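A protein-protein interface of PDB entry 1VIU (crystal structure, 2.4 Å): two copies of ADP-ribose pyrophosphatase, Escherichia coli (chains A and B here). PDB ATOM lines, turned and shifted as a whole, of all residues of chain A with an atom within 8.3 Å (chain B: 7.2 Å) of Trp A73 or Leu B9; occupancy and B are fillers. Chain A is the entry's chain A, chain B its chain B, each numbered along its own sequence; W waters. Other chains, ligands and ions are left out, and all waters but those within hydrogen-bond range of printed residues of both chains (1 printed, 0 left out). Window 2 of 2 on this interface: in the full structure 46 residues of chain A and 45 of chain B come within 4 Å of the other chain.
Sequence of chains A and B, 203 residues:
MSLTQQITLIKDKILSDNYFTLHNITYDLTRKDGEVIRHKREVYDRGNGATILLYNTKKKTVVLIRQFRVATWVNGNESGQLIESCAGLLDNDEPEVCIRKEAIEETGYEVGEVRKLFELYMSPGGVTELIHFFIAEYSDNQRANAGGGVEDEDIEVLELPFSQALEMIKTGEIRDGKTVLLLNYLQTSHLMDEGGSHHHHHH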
ATOM      1  N   PHE A  68      -8.069   5.472  21.614  1.00  0.00           N
ATOM      2  CA  PHE A  68      -7.638   5.838  22.943  1.00  0.00           C
ATOM      3  C   PHE A  68      -6.783   4.696  23.510  1.00  0.00           C
ATOM      4  O   PHE A  68      -7.159   3.524  23.454  1.00  0.00           O
ATOM      5  CB  PHE A  68      -8.848   6.079  23.844  1.00  0.00           C
ATOM      6  CG  PHE A  68      -8.480   6.405  25.267  1.00  0.00           C
ATOM      7  CD1 PHE A  68      -7.973   7.661  25.601  1.00  0.00           C
ATOM      8  CD2 PHE A  68      -8.581   5.435  26.265  1.00  0.00           C
ATOM      9  CE1 PHE A  68      -7.556   7.943  26.912  1.00  0.00           C
ATOM     10  CE2 PHE A  68      -8.168   5.713  27.572  1.00  0.00           C
ATOM     11  CZ  PHE A  68      -7.656   6.970  27.894  1.00  0.00           C
ATOM     12  N   ARG A  69      -5.615   5.053  24.031  1.00  0.00           N
ATOM     13  CA  ARG A  69      -4.699   4.086  24.636  1.00  0.00           C
ATOM     14  C   ARG A  69      -4.345   4.568  26.038  1.00  0.00           C
ATOM     15  O   ARG A  69      -3.480   5.444  26.178  1.00  0.00           O
ATOM     16  CB  ARG A  69      -3.418   3.974  23.809  1.00  0.00           C
ATOM     17  CG  ARG A  69      -3.574   3.280  22.476  1.00  0.00           C
ATOM     18  CD  ARG A  69      -4.005   1.834  22.645  1.00  0.00           C
ATOM     19  NE  ARG A  69      -3.523   1.049  21.527  1.00  0.00           N
ATOM     20  CZ  ARG A  69      -3.755  -0.247  21.349  1.00  0.00           C
ATOM     21  NH1 ARG A  69      -4.480  -0.939  22.220  1.00  0.00           N
ATOM     22  NH2 ARG A  69      -3.239  -0.858  20.299  1.00  0.00           N
ATOM     23  N   VAL A  70      -4.996   4.010  27.067  1.00  0.00           N
ATOM     24  CA  VAL A  70      -4.720   4.428  28.459  1.00  0.00           C
ATOM     25  C   VAL A  70      -3.257   4.433  28.838  1.00  0.00           C
ATOM     26  O   VAL A  70      -2.815   5.299  29.588  1.00  0.00           O
ATOM     27  CB  VAL A  70      -5.368   3.532  29.544  1.00  0.00           C
ATOM     28  CG1 VAL A  70      -6.618   4.158  30.046  1.00  0.00           C
ATOM     29  CG2 VAL A  70      -5.563   2.131  29.033  1.00  0.00           C
ATOM     30  N   ALA A  71      -2.520   3.441  28.353  1.00  0.00           N
ATOM     31  CA  ALA A  71      -1.111   3.332  28.693  1.00  0.00           C
ATOM     32  C   ALA A  71      -0.303   4.544  28.236  1.00  0.00           C
ATOM     33  O   ALA A  71       0.730   4.850  28.828  1.00  0.00           O
ATOM     34  CB  ALA A  71      -0.531   2.054  28.122  1.00  0.00           C
ATOM     35  N   THR A  72      -0.759   5.233  27.194  1.00  0.00           N
ATOM     36  CA  THR A  72      -0.035   6.415  26.744  1.00  0.00           C
ATOM     37  C   THR A  72      -0.637   7.615  27.460  1.00  0.00           C
ATOM     38  O   THR A  72       0.050   8.595  27.738  1.00  0.00           O
ATOM     39  CB  THR A  72      -0.143   6.650  25.202  1.00  0.00           C
ATOM     40  OG1 THR A  72      -1.494   6.982  24.841  1.00  0.00           O
ATOM     41  CG2 THR A  72       0.303   5.421  24.439  1.00  0.00           C
ATOM     42  N   TRP A  73      -1.924   7.513  27.772  1.00  0.00           N
ATOM     43  CA  TRP A  73      -2.648   8.587  28.448  1.00  0.00           C
ATOM     44  C   TRP A  73      -2.042   8.918  29.817  1.00  0.00           C
ATOM     45  O   TRP A  73      -1.961  10.083  30.203  1.00  0.00           O
ATOM     46  CB  TRP A  73      -4.120   8.191  28.605  1.00  0.00           C
ATOM     47  CG  TRP A  73      -4.999   9.289  29.113  1.00  0.00           C
ATOM     48  CD1 TRP A  73      -5.129  10.546  28.589  1.00  0.00           C
ATOM     49  CD2 TRP A  73      -5.901   9.221  30.225  1.00  0.00           C
ATOM     50  NE1 TRP A  73      -6.054  11.263  29.303  1.00  0.00           N
ATOM     51  CE2 TRP A  73      -6.544  10.479  30.312  1.00  0.00           C
ATOM     52  CE3 TRP A  73      -6.229   8.222  31.153  1.00  0.00           C
ATOM     53  CZ2 TRP A  73      -7.504  10.765  31.299  1.00  0.00           C
ATOM     54  CZ3 TRP A  73      -7.187   8.505  32.138  1.00  0.00           C
ATOM     55  CH2 TRP A  73      -7.811   9.771  32.200  1.00  0.00           C
ATOM     56  N   VAL A  74      -1.613   7.892  30.542  1.00  0.00           N
ATOM     57  CA  VAL A  74      -1.019   8.099  31.857  1.00  0.00           C
ATOM     58  C   VAL A  74       0.483   8.306  31.739  1.00  0.00           C
ATOM     59  O   VAL A  74       1.200   8.238  32.739  1.00  0.00           O
ATOM     60  CB  VAL A  74      -1.257   6.888  32.788  1.00  0.00           C
ATOM     61  CG1 VAL A  74      -2.745   6.571  32.869  1.00  0.00           C
ATOM     62  CG2 VAL A  74      -0.491   5.686  32.279  1.00  0.00           C
ATOM     63  N   ASN A  75       0.961   8.558  30.523  1.00  0.00           N
ATOM     64  CA  ASN A  75       2.387   8.759  30.315  1.00  0.00           C
ATOM     65  C   ASN A  75       2.749   9.672  29.146  1.00  0.00           C
ATOM     66  O   ASN A  75       3.464   9.264  28.223  1.00  0.00           O
ATOM     67  CB  ASN A  75       3.083   7.400  30.146  1.00  0.00           C
ATOM     68  CG  ASN A  75       4.597   7.519  30.086  1.00  0.00           C
ATOM     69  OD1 ASN A  75       5.209   8.189  30.917  1.00  0.00           O
ATOM     70  ND2 ASN A  75       5.210   6.859  29.105  1.00  0.00           N
ATOM     71  N   GLY A  76       2.243  10.904  29.180  1.00  0.00           N
ATOM     72  CA  GLY A  76       2.582  11.875  28.152  1.00  0.00           C
ATOM     73  C   GLY A  76       1.655  12.147  26.980  1.00  0.00           C
ATOM     74  O   GLY A  76       1.851  13.136  26.265  1.00  0.00           O
ATOM     75  N   ASN A  77       0.668  11.288  26.752  1.00  0.00           N
ATOM     76  CA  ASN A  77      -0.254  11.502  25.646  1.00  0.00           C
ATOM     77  C   ASN A  77      -1.530  12.101  26.218  1.00  0.00           C
ATOM     78  O   ASN A  77      -2.437  11.384  26.654  1.00  0.00           O
ATOM     79  CB  ASN A  77      -0.533  10.182  24.930  1.00  0.00           C
ATOM     80  CG  ASN A  77      -1.175  10.387  23.586  1.00  0.00           C
ATOM     81  OD1 ASN A  77      -1.099  11.473  23.016  1.00  0.00           O
ATOM     82  ND2 ASN A  77      -1.797   9.344  23.060  1.00  0.00           N
ATOM     83  N   GLU A  78      -1.575  13.431  26.208  1.00  0.00           N
ATOM     84  CA  GLU A  78      -2.680  14.211  26.757  1.00  0.00           C
ATOM     85  C   GLU A  78      -4.100  13.716  26.487  1.00  0.00           C
ATOM     86  O   GLU A  78      -4.864  13.486  27.427  1.00  0.00           O
ATOM     87  CB  GLU A  78      -2.558  15.666  26.301  1.00  0.00           C
ATOM     88  CG  GLU A  78      -3.030  16.665  27.346  1.00  0.00           C
ATOM     89  CD  GLU A  78      -2.861  18.100  26.899  1.00  0.00           C
ATOM     90  OE1 GLU A  78      -3.783  18.635  26.246  1.00  0.00           O
ATOM     91  OE2 GLU A  78      -1.798  18.690  27.189  1.00  0.00           O
ATOM     92  N   SER A  79      -4.467  13.570  25.218  1.00  0.00           N
ATOM     93  CA  SER A  79      -5.811  13.110  24.892  1.00  0.00           C
ATOM     94  C   SER A  79      -5.898  11.596  24.997  1.00  0.00           C
ATOM     95  O   SER A  79      -6.995  11.031  25.103  1.00  0.00           O
ATOM     96  CB  SER A  79      -6.201  13.534  23.469  1.00  0.00           C
ATOM     97  OG  SER A  79      -5.426  12.845  22.501  1.00  0.00           O
ATOM     98  N   GLY A  80      -4.738  10.941  24.957  1.00  0.00           N
ATOM     99  CA  GLY A  80      -4.717   9.492  25.019  1.00  0.00           C
ATOM    100  C   GLY A  80      -4.877   8.868  23.639  1.00  0.00           C
ATOM    101  O   GLY A  80      -4.629   7.669  23.470  1.00  0.00           O
ATOM    102  N   GLN A  81      -5.281   9.676  22.653  1.00  0.00           N
ATOM    103  CA  GLN A  81      -5.482   9.192  21.288  1.00  0.00           C
ATOM    104  C   GLN A  81      -4.155   8.854  20.609  1.00  0.00           C
ATOM    105  O   GLN A  81      -3.198   9.632  20.663  1.00  0.00           O
ATOM    106  CB  GLN A  81      -6.224  10.231  20.443  1.00  0.00           C
ATOM    107  CG  GLN A  81      -7.679  10.491  20.841  1.00  0.00           C
ATOM    108  CD  GLN A  81      -8.545   9.251  20.740  1.00  0.00           C
ATOM    109  OE1 GLN A  81      -8.456   8.504  19.774  1.00  0.00           O
ATOM    110  NE2 GLN A  81      -9.402   9.036  21.735  1.00  0.00           N
ATOM    111  N   LEU A  82      -4.105   7.696  19.961  1.00  0.00           N
ATOM    112  CA  LEU A  82      -2.888   7.273  19.292  1.00  0.00           C
ATOM    113  C   LEU A  82      -3.194   6.772  17.878  1.00  0.00           C
ATOM    114  O   LEU A  82      -4.113   5.984  17.679  1.00  0.00           O
ATOM    115  CB  LEU A  82      -2.216   6.167  20.112  1.00  0.00           C
ATOM    116  CG  LEU A  82      -0.746   5.876  19.841  1.00  0.00           C
ATOM    117  CD1 LEU A  82       0.104   7.047  20.288  1.00  0.00           C
ATOM    118  CD2 LEU A  82      -0.342   4.630  20.586  1.00  0.00           C
ATOM    119  N   ILE B   7     -13.150  11.216  28.316  1.00  0.00           N
ATOM    120  CA  ILE B   7     -12.595  10.073  29.019  1.00  0.00           C
ATOM    121  C   ILE B   7     -12.431  10.436  30.492  1.00  0.00           C
ATOM    122  O   ILE B   7     -11.912  11.502  30.836  1.00  0.00           O
ATOM    123  CB  ILE B   7     -11.233   9.659  28.403  1.00  0.00           C
ATOM    124  CG1 ILE B   7     -10.744   8.349  29.020  1.00  0.00           C
ATOM    125  CG2 ILE B   7     -10.218  10.769  28.583  1.00  0.00           C
ATOM    126  CD1 ILE B   7     -10.261   8.459  30.432  1.00  0.00           C
ATOM    127  N   THR B   8     -12.894   9.552  31.364  1.00  0.00           N
ATOM    128  CA  THR B   8     -12.801   9.782  32.794  1.00  0.00           C
ATOM    129  C   THR B   8     -12.145   8.608  33.514  1.00  0.00           C
ATOM    130  O   THR B   8     -12.544   7.459  33.336  1.00  0.00           O
ATOM    131  CB  THR B   8     -14.198   9.993  33.408  1.00  0.00           C
ATOM    132  OG1 THR B   8     -14.853  11.081  32.745  1.00  0.00           O
ATOM    133  CG2 THR B   8     -14.087  10.297  34.908  1.00  0.00           C
ATOM    134  N   LEU B   9     -11.139   8.906  34.331  1.00  0.00           N
ATOM    135  CA  LEU B   9     -10.451   7.879  35.105  1.00  0.00           C
ATOM    136  C   LEU B   9     -11.416   7.478  36.216  1.00  0.00           C
ATOM    137  O   LEU B   9     -11.949   8.338  36.907  1.00  0.00           O
ATOM    138  CB  LEU B   9      -9.154   8.448  35.694  1.00  0.00           C
ATOM    139  CG  LEU B   9      -8.407   7.592  36.724  1.00  0.00           C
ATOM    140  CD1 LEU B   9      -7.970   6.274  36.104  1.00  0.00           C
ATOM    141  CD2 LEU B   9      -7.203   8.365  37.254  1.00  0.00           C
ATOM    142  N   ILE B  10     -11.671   6.184  36.370  1.00  0.00           N
ATOM    143  CA  ILE B  10     -12.593   5.721  37.406  1.00  0.00           C
ATOM    144  C   ILE B  10     -11.825   5.183  38.614  1.00  0.00           C
ATOM    145  O   ILE B  10     -12.147   5.515  39.752  1.00  0.00           O
ATOM    146  CB  ILE B  10     -13.546   4.638  36.861  1.00  0.00           C
ATOM    147  CG1 ILE B  10     -14.408   5.219  35.728  1.00  0.00           C
ATOM    148  CG2 ILE B  10     -14.439   4.115  37.974  1.00  0.00           C
ATOM    149  CD1 ILE B  10     -15.321   6.371  36.150  1.00  0.00           C
ATOM    150  N   LYS B  11     -10.825   4.339  38.371  1.00  0.00           N
ATOM    151  CA  LYS B  11     -10.003   3.827  39.457  1.00  0.00           C
ATOM    152  C   LYS B  11      -8.686   3.248  38.968  1.00  0.00           C
ATOM    153  O   LYS B  11      -8.571   2.786  37.829  1.00  0.00           O
ATOM    154  CB  LYS B  11     -10.753   2.788  40.301  1.00  0.00           C
ATOM    155  CG  LYS B  11     -10.799   1.402  39.725  1.00  0.00           C
ATOM    156  CD  LYS B  11     -11.299   0.398  40.755  1.00  0.00           C
ATOM    157  CE  LYS B  11     -10.326   0.265  41.914  1.00  0.00           C
ATOM    158  NZ  LYS B  11     -10.675  -0.878  42.809  1.00  0.00           N
ATOM    159  N   ASP B  12      -7.688   3.300  39.842  1.00  0.00           N
ATOM    160  CA  ASP B  12      -6.366   2.790  39.534  1.00  0.00           C
ATOM    161  C   ASP B  12      -5.929   1.828  40.626  1.00  0.00           C
ATOM    162  O   ASP B  12      -5.445   2.232  41.679  1.00  0.00           O
ATOM    163  CB  ASP B  12      -5.375   3.956  39.395  1.00  0.00           C
ATOM    164  CG  ASP B  12      -3.941   3.489  39.176  1.00  0.00           C
ATOM    165  OD1 ASP B  12      -3.735   2.325  38.767  1.00  0.00           O
ATOM    166  OD2 ASP B  12      -3.017   4.296  39.410  1.00  0.00           O
ATOM    167  N   ASN B  24      -4.285  -1.761  37.087  1.00  0.00           N
ATOM    168  CA  ASN B  24      -5.496  -2.229  36.450  1.00  0.00           C
ATOM    169  C   ASN B  24      -6.256  -0.912  36.438  1.00  0.00           C
ATOM    170  O   ASN B  24      -6.715  -0.449  37.484  1.00  0.00           O
ATOM    171  CB  ASN B  24      -6.244  -3.247  37.309  1.00  0.00           C
ATOM    172  CG  ASN B  24      -6.964  -4.295  36.469  1.00  0.00           C
ATOM    173  OD1 ASN B  24      -7.287  -4.062  35.304  1.00  0.00           O
ATOM    174  ND2 ASN B  24      -7.223  -5.454  37.064  1.00  0.00           N
ATOM    175  N   ILE B  25      -6.349  -0.289  35.270  1.00  0.00           N
ATOM    176  CA  ILE B  25      -7.033   0.987  35.151  1.00  0.00           C
ATOM    177  C   ILE B  25      -8.434   0.871  34.596  1.00  0.00           C
ATOM    178  O   ILE B  25      -8.653   0.281  33.539  1.00  0.00           O
ATOM    179  CB  ILE B  25      -6.237   1.957  34.271  1.00  0.00           C
ATOM    180  CG1 ILE B  25      -4.840   2.150  34.872  1.00  0.00           C
ATOM    181  CG2 ILE B  25      -6.965   3.298  34.180  1.00  0.00           C
ATOM    182  CD1 ILE B  25      -3.964   3.110  34.133  1.00  0.00           C
ATOM    183  N   THR B  26      -9.383   1.436  35.331  1.00  0.00           N
ATOM    184  CA  THR B  26     -10.780   1.433  34.933  1.00  0.00           C
ATOM    185  C   THR B  26     -11.128   2.845  34.488  1.00  0.00           C
ATOM    186  O   THR B  26     -10.921   3.808  35.236  1.00  0.00           O
ATOM    187  CB  THR B  26     -11.680   1.058  36.108  1.00  0.00           C
ATOM    188  OG1 THR B  26     -11.283  -0.216  36.609  1.00  0.00           O
ATOM    189  CG2 THR B  26     -13.146   0.998  35.680  1.00  0.00           C
ATOM    190  N   TYR B  27     -11.649   2.974  33.273  1.00  0.00           N
ATOM    191  CA  TYR B  27     -12.005   4.292  32.768  1.00  0.00           C
ATOM    192  C   TYR B  27     -13.303   4.307  31.954  1.00  0.00           C
ATOM    193  O   TYR B  27     -13.743   3.281  31.430  1.00  0.00           O
ATOM    194  CB  TYR B  27     -10.844   4.866  31.941  1.00  0.00           C
ATOM    195  CG  TYR B  27     -10.507   4.091  30.695  1.00  0.00           C
ATOM    196  CD1 TYR B  27     -11.168   4.343  29.490  1.00  0.00           C
ATOM    197  CD2 TYR B  27      -9.529   3.099  30.715  1.00  0.00           C
ATOM    198  CE1 TYR B  27     -10.855   3.618  28.327  1.00  0.00           C
ATOM    199  CE2 TYR B  27      -9.209   2.370  29.570  1.00  0.00           C
ATOM    200  CZ  TYR B  27      -9.876   2.632  28.379  1.00  0.00           C
ATOM    201  OH  TYR B  27      -9.583   1.885  27.261  1.00  0.00           O
ATOM    202  N   ASP B  28     -13.924   5.482  31.895  1.00  0.00           N
ATOM    203  CA  ASP B  28     -15.161   5.690  31.158  1.00  0.00           C
ATOM    204  C   ASP B  28     -14.891   6.608  29.978  1.00  0.00           C
ATOM    205  O   ASP B  28     -14.333   7.696  30.130  1.00  0.00           O
ATOM    206  CB  ASP B  28     -16.227   6.338  32.049  1.00  0.00           C
ATOM    207  CG  ASP B  28     -16.847   5.360  33.027  1.00  0.00           C
ATOM    208  OD1 ASP B  28     -16.455   4.183  33.014  1.00  0.00           O
ATOM    209  OD2 ASP B  28     -17.729   5.772  33.812  1.00  0.00           O
ATOM    210  N   TYR B 121       6.163   5.134  21.562  1.00  0.00           N
ATOM    211  CA  TYR B 121       5.609   4.123  22.448  1.00  0.00           C
ATOM    212  C   TYR B 121       5.891   2.815  21.687  1.00  0.00           C
ATOM    213  O   TYR B 121       5.547   2.692  20.518  1.00  0.00           O
ATOM    214  CB  TYR B 121       4.101   4.344  22.637  1.00  0.00           C
ATOM    215  CG  TYR B 121       3.787   5.627  23.380  1.00  0.00           C
ATOM    216  CD1 TYR B 121       3.386   6.770  22.700  1.00  0.00           C
ATOM    217  CD2 TYR B 121       3.944   5.707  24.764  1.00  0.00           C
ATOM    218  CE1 TYR B 121       3.150   7.963  23.378  1.00  0.00           C
ATOM    219  CE2 TYR B 121       3.713   6.893  25.451  1.00  0.00           C
ATOM    220  CZ  TYR B 121       3.314   8.018  24.755  1.00  0.00           C
ATOM    221  OH  TYR B 121       3.082   9.198  25.435  1.00  0.00           O
ATOM    222  N   THR B 128       3.401   1.472  29.241  1.00  0.00           N
ATOM    223  CA  THR B 128       3.550   2.921  29.159  1.00  0.00           C
ATOM    224  C   THR B 128       4.830   3.296  28.420  1.00  0.00           C
ATOM    225  O   THR B 128       4.914   4.353  27.814  1.00  0.00           O
ATOM    226  CB  THR B 128       3.645   3.550  30.571  1.00  0.00           C
ATOM    227  OG1 THR B 128       4.696   2.899  31.301  1.00  0.00           O
ATOM    228  CG2 THR B 128       2.346   3.394  31.338  1.00  0.00           C
HETATM  229  O   HOH W   1      -6.914   1.857  26.202  1.00  0.00           O
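The side-chain hydroxyl (OH) of Tyr B121 lies within hydrogen-bond range of the backbone carbonyl oxygen (O) of Asn A75, at 2.8 Å. ND2 of Asn A75 is in hydrogen-bond range of O of Thr B128 (2.8 Å). N of Asn A77 lies within hydrogen-bond range of OH of Tyr B121 (3.5 Å).
O of Thr A72 is in hydrogen-bond range of N of Asn A77. O of Gln A81 lies within hydrogen-bond range of ND2 of Asn A77 (2.8 Å). The side-chain hydroxyl of Thr A72 sits at hydrogen-bond distance from the backbone carbonyl oxygen of Gly A80 (3.5 Å). The side-chain amide nitrogen (ND2) of Asn A77 lies close to the backbone carbonyl oxygen (O) of Gly A80. The side-chain hydroxyl (OG1) of Thr A72 sits at hydrogen-bond distance from the backbone carbonyl oxygen (O) of Arg A69, 2.8 Å away. The backbone carbonyl oxygen (O) of Glu A78 is in hydrogen-bond range of the indole nitrogen (NE1) of Trp A73 (3.1 Å).
Among the printed residues, pairs that only touch across the chains: Val A70 with Tyr B27 (3.2 Å), Trp A73 with Ile B7 (3.3 Å), Ala A71 with Thr B128 (3.3 Å), Phe A68 with Tyr B27 (3.5 Å), Phe A68 with Ile B7 (3.6 Å), Gly A76 with Tyr B121 (3.6 Å), Thr A72 with Tyr B121 (3.6 Å), Val A74 with Thr B128 (3.8 Å), Val A74 with Ile B25 (3.9 Å) and Trp A73 with Leu B9 (3.97 Å).
Of the printed residues of chain B, Trp A73 touches Ile B7 (3.3 Å) and Leu B9 (3.97 Å). Leu B9 touches one residue of chain A. Of the printed residues of chain A, Ile B7 touches Phe A68 (3.6 Å) and Trp A73 (3.3 Å). Of the printed residues of chain B, Phe A68 touches Ile B7 and Tyr B27. Printed residues of chain B within 4 Å of Ala A71: Thr B128 (3.3 Å). Printed residues of chain B within 4 Å of Val A74: Ile B25 (3.9 Å) and Thr B128 (3.8 Å). Printed residues of chain A within 4 Å of Tyr B27: Phe A68 and Val A70. Asn B24 touches none of the printed residues of chain A.
Of the 15 printed residues of chain A, 9 touch a printed residue of chain B. Printed residues of chain A that touch a printed residue of chain B: Phe A68, Val A70, Ala A71, Thr A72, Trp A73, Val A74, Asn A75, Gly A76 and Asn A77. Of the 13 printed residues of chain B, 6 touch a printed residue of chain A. Hydrophobic or aromatic side chains of chain B that line the printed part of chain A: Ile B7, Leu B9, Ile B25, Tyr B27 and Tyr B121.
No position is printed for both chains. Of the 13 pairs that touch across the chains among the printed residues, none has its exchanged pair printed and touching as well.
Water W1 lies within hydrogen-bond range of the side-chain hydroxyl (OH) of Tyr B27, the backbone NH (N) of Val A70 and the backbone carbonyl oxygen (O) of Phe A68.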
